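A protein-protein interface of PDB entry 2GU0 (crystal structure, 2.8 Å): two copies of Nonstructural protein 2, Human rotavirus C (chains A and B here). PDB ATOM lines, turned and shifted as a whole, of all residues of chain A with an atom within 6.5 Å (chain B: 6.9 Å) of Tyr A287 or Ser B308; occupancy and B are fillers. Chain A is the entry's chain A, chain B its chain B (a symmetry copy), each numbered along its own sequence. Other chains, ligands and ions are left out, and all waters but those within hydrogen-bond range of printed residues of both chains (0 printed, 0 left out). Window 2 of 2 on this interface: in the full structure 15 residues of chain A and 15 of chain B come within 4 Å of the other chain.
A ring nitrogen (NE2) of His A228 sits close to the side-chain carboxylate (OE2) of Glu B303, at 3.3 Å.
The backbone carbonyl oxygen (O) of Asn B300 lies within hydrogen-bond range of the side-chain hydroxyl (OG) of Ser B304 (3.2 Å).
Among the printed residues, pairs that only touch across the chains: His A228 with Leu B306 (3.7 Å), His A228 with Ile B307 (3.3 Å), Leu A231 with Ile B307 (3.8 Å), Met A232 with Ile B307 (3.2 Å), Tyr A287 with Ser B304 (3.6 Å), Tyr A287 with Ile B307 (3.7 Å) and Tyr A287 with Ser B308 (3.1 Å).
Of the printed residues of chain B, Tyr A287 touches Ser B304 (3.6 Å), Ile B307 (3.7 Å) and Ser B308 (3.1 Å). Of chain A, only Tyr A287 comes within 4 Å of Ser B308. Of the printed residues of chain A, Glu B303 touches His A228. Of the printed residues of chain A, Leu B306 touches His A228 (3.7 Å). The nearest printed residue of chain A that does not touch Glu B303 is His A263 (4.8 Å).
Hydrophobic or aromatic side chains of chain A within 4 Å of the printed part of chain B: His A228, Leu A231, Met A232 and Tyr A287. Of the 8 printed residues of chain B, 5 touch a printed residue of chain A. Printed residues of chain B that touch a printed residue of chain A: Glu B303, Ser B304, Leu B306, Ile B307 and Ser B308. Hydrophobic or aromatic side chains of chain B that line the printed part of chain A: Ile B307. Among the printed residues, no Asp or Glu carboxylate lies within 4 Å of a Lys or Arg side-chain nitrogen of the other chain.
No position is printed for both chains. Of the 8 pairs that touch across the chains among the printed residues, none has its exchanged pair printed and touching as well.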
ATOM      1  N   HIS A 228      10.351 -22.337 -11.132  1.00  0.00           N
ATOM      2  CA  HIS A 228      11.449 -23.138 -10.594  1.00  0.00           C
ATOM      3  C   HIS A 228      12.666 -22.986 -11.506  1.00  0.00           C
ATOM      4  O   HIS A 228      13.809 -22.937 -11.043  1.00  0.00           O
ATOM      5  CB  HIS A 228      11.051 -24.614 -10.499  1.00  0.00           C
ATOM      6  CG  HIS A 228      10.027 -24.905  -9.442  1.00  0.00           C
ATOM      7  ND1 HIS A 228      10.148 -24.459  -8.144  1.00  0.00           N
ATOM      8  CD2 HIS A 228       8.884 -25.631  -9.483  1.00  0.00           C
ATOM      9  CE1 HIS A 228       9.125 -24.898  -7.432  1.00  0.00           C
ATOM     10  NE2 HIS A 228       8.345 -25.612  -8.221  1.00  0.00           N
ATOM     11  N   LEU A 231      14.559 -20.013 -10.179  1.00  0.00           N
ATOM     12  CA  LEU A 231      14.972 -19.968  -8.789  1.00  0.00           C
ATOM     13  C   LEU A 231      16.466 -19.644  -8.646  1.00  0.00           C
ATOM     14  O   LEU A 231      16.840 -18.831  -7.803  1.00  0.00           O
ATOM     15  CB  LEU A 231      14.610 -21.299  -8.117  1.00  0.00           C
ATOM     16  CG  LEU A 231      14.482 -21.323  -6.594  1.00  0.00           C
ATOM     17  CD1 LEU A 231      13.767 -20.076  -6.093  1.00  0.00           C
ATOM     18  CD2 LEU A 231      13.729 -22.571  -6.187  1.00  0.00           C
ATOM     19  N   MET A 232      17.312 -20.263  -9.472  1.00  0.00           N
ATOM     20  CA  MET A 232      18.752 -19.996  -9.425  1.00  0.00           C
ATOM     21  C   MET A 232      19.030 -18.507  -9.623  1.00  0.00           C
ATOM     22  O   MET A 232      19.540 -17.837  -8.728  1.00  0.00           O
ATOM     23  CB  MET A 232      19.490 -20.787 -10.508  1.00  0.00           C
ATOM     24  CG  MET A 232      19.857 -22.209 -10.115  1.00  0.00           C
ATOM     25  SD  MET A 232      21.033 -22.295  -8.745  1.00  0.00           S
ATOM     26  CE  MET A 232      22.525 -21.878  -9.619  1.00  0.00           C
ATOM     27  N   HIS A 263       9.568 -20.652  -0.070  1.00  0.00           N
ATOM     28  CA  HIS A 263      10.240 -21.846  -0.569  1.00  0.00           C
ATOM     29  C   HIS A 263      11.431 -22.261   0.298  1.00  0.00           C
ATOM     30  O   HIS A 263      12.458 -21.574   0.335  1.00  0.00           O
ATOM     31  CB  HIS A 263      10.699 -21.599  -1.999  1.00  0.00           C
ATOM     32  CG  HIS A 263      11.396 -22.766  -2.609  1.00  0.00           C
ATOM     33  ND1 HIS A 263      12.581 -23.259  -2.114  1.00  0.00           N
ATOM     34  CD2 HIS A 263      11.069 -23.549  -3.661  1.00  0.00           C
ATOM     35  CE1 HIS A 263      12.954 -24.298  -2.836  1.00  0.00           C
ATOM     36  NE2 HIS A 263      12.054 -24.495  -3.781  1.00  0.00           N
ATOM     37  N   GLY A 265      13.962 -24.354   0.107  1.00  0.00           N
ATOM     38  CA  GLY A 265      15.281 -24.318  -0.494  1.00  0.00           C
ATOM     39  C   GLY A 265      15.855 -22.922  -0.400  1.00  0.00           C
ATOM     40  O   GLY A 265      16.993 -22.731   0.035  1.00  0.00           O
ATOM     41  N   TRP A 266      15.049 -21.944  -0.800  1.00  0.00           N
ATOM     42  CA  TRP A 266      15.438 -20.544  -0.769  1.00  0.00           C
ATOM     43  C   TRP A 266      15.731 -20.144   0.669  1.00  0.00           C
ATOM     44  O   TRP A 266      16.786 -19.606   0.967  1.00  0.00           O
ATOM     45  CB  TRP A 266      14.297 -19.693  -1.341  1.00  0.00           C
ATOM     46  CG  TRP A 266      14.580 -18.206  -1.433  1.00  0.00           C
ATOM     47  CD1 TRP A 266      14.274 -17.249  -0.505  1.00  0.00           C
ATOM     48  CD2 TRP A 266      15.221 -17.522  -2.516  1.00  0.00           C
ATOM     49  NE1 TRP A 266      14.683 -16.020  -0.945  1.00  0.00           N
ATOM     50  CE2 TRP A 266      15.268 -16.156  -2.175  1.00  0.00           C
ATOM     51  CE3 TRP A 266      15.759 -17.935  -3.740  1.00  0.00           C
ATOM     52  CZ2 TRP A 266      15.833 -15.196  -3.015  1.00  0.00           C
ATOM     53  CZ3 TRP A 266      16.323 -16.983  -4.575  1.00  0.00           C
ATOM     54  CH2 TRP A 266      16.355 -15.626  -4.209  1.00  0.00           C
ATOM     55  N   LYS A 283      23.957 -22.983  -3.211  1.00  0.00           N
ATOM     56  CA  LYS A 283      23.057 -23.106  -4.352  1.00  0.00           C
ATOM     57  C   LYS A 283      22.443 -24.496  -4.386  1.00  0.00           C
ATOM     58  O   LYS A 283      21.489 -24.742  -5.106  1.00  0.00           O
ATOM     59  CB  LYS A 283      23.805 -22.873  -5.662  1.00  0.00           C
ATOM     60  CG  LYS A 283      24.694 -24.033  -6.056  1.00  0.00           C
ATOM     61  CD  LYS A 283      25.044 -24.020  -7.543  1.00  0.00           C
ATOM     62  CE  LYS A 283      26.024 -22.920  -7.895  1.00  0.00           C
ATOM     63  NZ  LYS A 283      26.267 -22.881  -9.359  1.00  0.00           N
ATOM     64  N   THR A 284      23.001 -25.404  -3.599  1.00  0.00           N
ATOM     65  CA  THR A 284      22.526 -26.779  -3.546  1.00  0.00           C
ATOM     66  C   THR A 284      21.238 -26.949  -2.759  1.00  0.00           C
ATOM     67  O   THR A 284      20.305 -27.602  -3.222  1.00  0.00           O
ATOM     68  CB  THR A 284      23.612 -27.697  -2.939  1.00  0.00           C
ATOM     69  OG1 THR A 284      24.728 -27.747  -3.833  1.00  0.00           O
ATOM     70  CG2 THR A 284      23.078 -29.110  -2.702  1.00  0.00           C
ATOM     71  N   SER A 285      21.187 -26.366  -1.569  1.00  0.00           N
ATOM     72  CA  SER A 285      20.006 -26.488  -0.726  1.00  0.00           C
ATOM     73  C   SER A 285      18.739 -25.897  -1.346  1.00  0.00           C
ATOM     74  O   SER A 285      17.665 -25.988  -0.763  1.00  0.00           O
ATOM     75  CB  SER A 285      20.276 -25.865   0.652  1.00  0.00           C
ATOM     76  OG  SER A 285      21.050 -24.681   0.548  1.00  0.00           O
ATOM     77  N   LEU A 286      18.871 -25.306  -2.532  1.00  0.00           N
ATOM     78  CA  LEU A 286      17.737 -24.712  -3.241  1.00  0.00           C
ATOM     79  C   LEU A 286      16.779 -25.759  -3.797  1.00  0.00           C
ATOM     80  O   LEU A 286      15.570 -25.558  -3.812  1.00  0.00           O
ATOM     81  CB  LEU A 286      18.223 -23.859  -4.414  1.00  0.00           C
ATOM     82  CG  LEU A 286      18.773 -22.461  -4.171  1.00  0.00           C
ATOM     83  CD1 LEU A 286      19.143 -21.850  -5.511  1.00  0.00           C
ATOM     84  CD2 LEU A 286      17.734 -21.610  -3.461  1.00  0.00           C
ATOM     85  N   TYR A 287      17.328 -26.871  -4.268  1.00  0.00           N
ATOM     86  CA  TYR A 287      16.524 -27.935  -4.849  1.00  0.00           C
ATOM     87  C   TYR A 287      16.652 -29.218  -4.055  1.00  0.00           C
ATOM     88  O   TYR A 287      16.036 -30.225  -4.394  1.00  0.00           O
ATOM     89  CB  TYR A 287      16.991 -28.188  -6.269  1.00  0.00           C
ATOM     90  CG  TYR A 287      18.473 -28.441  -6.322  1.00  0.00           C
ATOM     91  CD1 TYR A 287      18.998 -29.692  -6.010  1.00  0.00           C
ATOM     92  CD2 TYR A 287      19.358 -27.414  -6.629  1.00  0.00           C
ATOM     93  CE1 TYR A 287      20.375 -29.910  -6.001  1.00  0.00           C
ATOM     94  CE2 TYR A 287      20.736 -27.623  -6.623  1.00  0.00           C
ATOM     95  CZ  TYR A 287      21.237 -28.871  -6.308  1.00  0.00           C
ATOM     96  OH  TYR A 287      22.598 -29.068  -6.290  1.00  0.00           O
ATOM     97  N   SER A 288      17.458 -29.190  -3.004  1.00  0.00           N
ATOM     98  CA  SER A 288      17.651 -30.381  -2.198  1.00  0.00           C
ATOM     99  C   SER A 288      16.824 -30.424  -0.915  1.00  0.00           C
ATOM    100  O   SER A 288      16.838 -31.432  -0.210  1.00  0.00           O
ATOM    101  CB  SER A 288      19.133 -30.555  -1.869  1.00  0.00           C
ATOM    102  OG  SER A 288      19.616 -29.445  -1.141  1.00  0.00           O
ATOM    103  N   ILE A 289      16.105 -29.345  -0.603  1.00  0.00           N
ATOM    104  CA  ILE A 289      15.272 -29.332   0.600  1.00  0.00           C
ATOM    105  C   ILE A 289      13.785 -29.498   0.280  1.00  0.00           C
ATOM    106  O   ILE A 289      13.263 -28.850  -0.624  1.00  0.00           O
ATOM    107  CB  ILE A 289      15.466 -28.050   1.409  1.00  0.00           C
ATOM    108  CG1 ILE A 289      16.861 -28.050   2.027  1.00  0.00           C
ATOM    109  CG2 ILE A 289      14.404 -27.952   2.494  1.00  0.00           C
ATOM    110  CD1 ILE A 289      17.090 -26.941   3.023  1.00  0.00           C
ATOM    111  N   LYS A 290      13.113 -30.369   1.035  1.00  0.00           N
ATOM    112  CA  LYS A 290      11.688 -30.659   0.843  1.00  0.00           C
ATOM    113  C   LYS A 290      10.791 -29.757   1.689  1.00  0.00           C
ATOM    114  O   LYS A 290      11.212 -29.244   2.726  1.00  0.00           O
ATOM    115  CB  LYS A 290      11.400 -32.116   1.220  1.00  0.00           C
ATOM    116  CG  LYS A 290      12.483 -33.094   0.792  1.00  0.00           C
ATOM    117  CD  LYS A 290      12.336 -34.448   1.472  1.00  0.00           C
ATOM    118  CE  LYS A 290      13.568 -35.323   1.223  1.00  0.00           C
ATOM    119  NZ  LYS A 290      13.524 -36.611   1.989  1.00  0.00           N
ATOM    120  N   ASN B 300       8.784 -34.909  -8.529  1.00  0.00           N
ATOM    121  CA  ASN B 300       9.686 -34.043  -7.790  1.00  0.00           C
ATOM    122  C   ASN B 300      11.008 -33.932  -8.542  1.00  0.00           C
ATOM    123  O   ASN B 300      11.714 -32.928  -8.430  1.00  0.00           O
ATOM    124  CB  ASN B 300       9.935 -34.596  -6.389  1.00  0.00           C
ATOM    125  CG  ASN B 300       8.647 -34.864  -5.633  1.00  0.00           C
ATOM    126  OD1 ASN B 300       7.718 -34.053  -5.657  1.00  0.00           O
ATOM    127  ND2 ASN B 300       8.588 -36.002  -4.944  1.00  0.00           N
ATOM    128  N   GLU B 303      10.957 -31.138 -11.119  1.00  0.00           N
ATOM    129  CA  GLU B 303      11.010 -29.861 -10.429  1.00  0.00           C
ATOM    130  C   GLU B 303      12.402 -29.434 -10.011  1.00  0.00           C
ATOM    131  O   GLU B 303      12.849 -28.350 -10.367  1.00  0.00           O
ATOM    132  CB  GLU B 303      10.113 -29.890  -9.199  1.00  0.00           C
ATOM    133  CG  GLU B 303       9.885 -28.520  -8.622  1.00  0.00           C
ATOM    134  CD  GLU B 303       9.228 -28.551  -7.271  1.00  0.00           C
ATOM    135  OE1 GLU B 303       8.182 -29.216  -7.130  1.00  0.00           O
ATOM    136  OE2 GLU B 303       9.756 -27.902  -6.347  1.00  0.00           O
ATOM    137  N   SER B 304      13.085 -30.273  -9.240  1.00  0.00           N
ATOM    138  CA  SER B 304      14.429 -29.940  -8.789  1.00  0.00           C
ATOM    139  C   SER B 304      15.416 -29.936  -9.949  1.00  0.00           C
ATOM    140  O   SER B 304      16.467 -29.306  -9.856  1.00  0.00           O
ATOM    141  CB  SER B 304      14.888 -30.923  -7.724  1.00  0.00           C
ATOM    142  OG  SER B 304      14.839 -32.236  -8.236  1.00  0.00           O
ATOM    143  N   ASP B 305      15.101 -30.648 -11.029  1.00  0.00           N
ATOM    144  CA  ASP B 305      15.985 -30.642 -12.195  1.00  0.00           C
ATOM    145  C   ASP B 305      15.868 -29.267 -12.846  1.00  0.00           C
ATOM    146  O   ASP B 305      16.847 -28.726 -13.352  1.00  0.00           O
ATOM    147  CB  ASP B 305      15.599 -31.719 -13.223  1.00  0.00           C
ATOM    148  CG  ASP B 305      16.235 -33.072 -12.933  1.00  0.00           C
ATOM    149  OD1 ASP B 305      17.132 -33.148 -12.061  1.00  0.00           O
ATOM    150  OD2 ASP B 305      15.840 -34.061 -13.589  1.00  0.00           O
ATOM    151  N   LEU B 306      14.659 -28.711 -12.832  1.00  0.00           N
ATOM    152  CA  LEU B 306      14.411 -27.394 -13.402  1.00  0.00           C
ATOM    153  C   LEU B 306      15.099 -26.350 -12.533  1.00  0.00           C
ATOM    154  O   LEU B 306      15.692 -25.405 -13.044  1.00  0.00           O
ATOM    155  CB  LEU B 306      12.902 -27.118 -13.485  1.00  0.00           C
ATOM    156  CG  LEU B 306      12.158 -27.546 -14.765  1.00  0.00           C
ATOM    157  CD1 LEU B 306      10.669 -27.659 -14.517  1.00  0.00           C
ATOM    158  CD2 LEU B 306      12.420 -26.538 -15.858  1.00  0.00           C
ATOM    159  N   ILE B 307      15.031 -26.533 -11.220  1.00  0.00           N
ATOM    160  CA  ILE B 307      15.666 -25.602 -10.294  1.00  0.00           C
ATOM    161  C   ILE B 307      17.172 -25.699 -10.430  1.00  0.00           C
ATOM    162  O   ILE B 307      17.871 -24.692 -10.497  1.00  0.00           O
ATOM    163  CB  ILE B 307      15.357 -25.939  -8.832  1.00  0.00           C
ATOM    164  CG1 ILE B 307      13.848 -25.918  -8.579  1.00  0.00           C
ATOM    165  CG2 ILE B 307      16.093 -24.965  -7.924  1.00  0.00           C
ATOM    166  CD1 ILE B 307      13.467 -26.336  -7.161  1.00  0.00           C
ATOM    167  N   SER B 308      17.651 -26.939 -10.464  1.00  0.00           N
ATOM    168  CA  SER B 308      19.069 -27.266 -10.552  1.00  0.00           C
ATOM    169  C   SER B 308      19.491 -27.743 -11.935  1.00  0.00           C
ATOM    170  O   SER B 308      19.513 -28.951 -12.182  1.00  0.00           O
ATOM    171  CB  SER B 308      19.382 -28.368  -9.537  1.00  0.00           C
ATOM    172  OG  SER B 308      20.750 -28.727  -9.541  1.00  0.00           O
ATOM    173  N   MET B 309      19.829 -26.809 -12.823  1.00  0.00           N
ATOM    174  CA  MET B 309      20.266 -27.140 -14.181  1.00  0.00           C
ATOM    175  C   MET B 309      19.992 -25.982 -15.127  1.00  0.00           C
ATOM    176  O   MET B 309      19.330 -26.222 -16.161  1.00  0.00           O
ATOM    177  CB  MET B 309      19.538 -28.381 -14.692  1.00  0.00           C
ATOM    178  CG  MET B 309      20.255 -29.122 -15.792  1.00  0.00           C
ATOM    179  SD  MET B 309      19.412 -30.674 -16.159  1.00  0.00           S
ATOM    180  CE  MET B 309      19.679 -31.558 -14.625  1.00  0.00           C
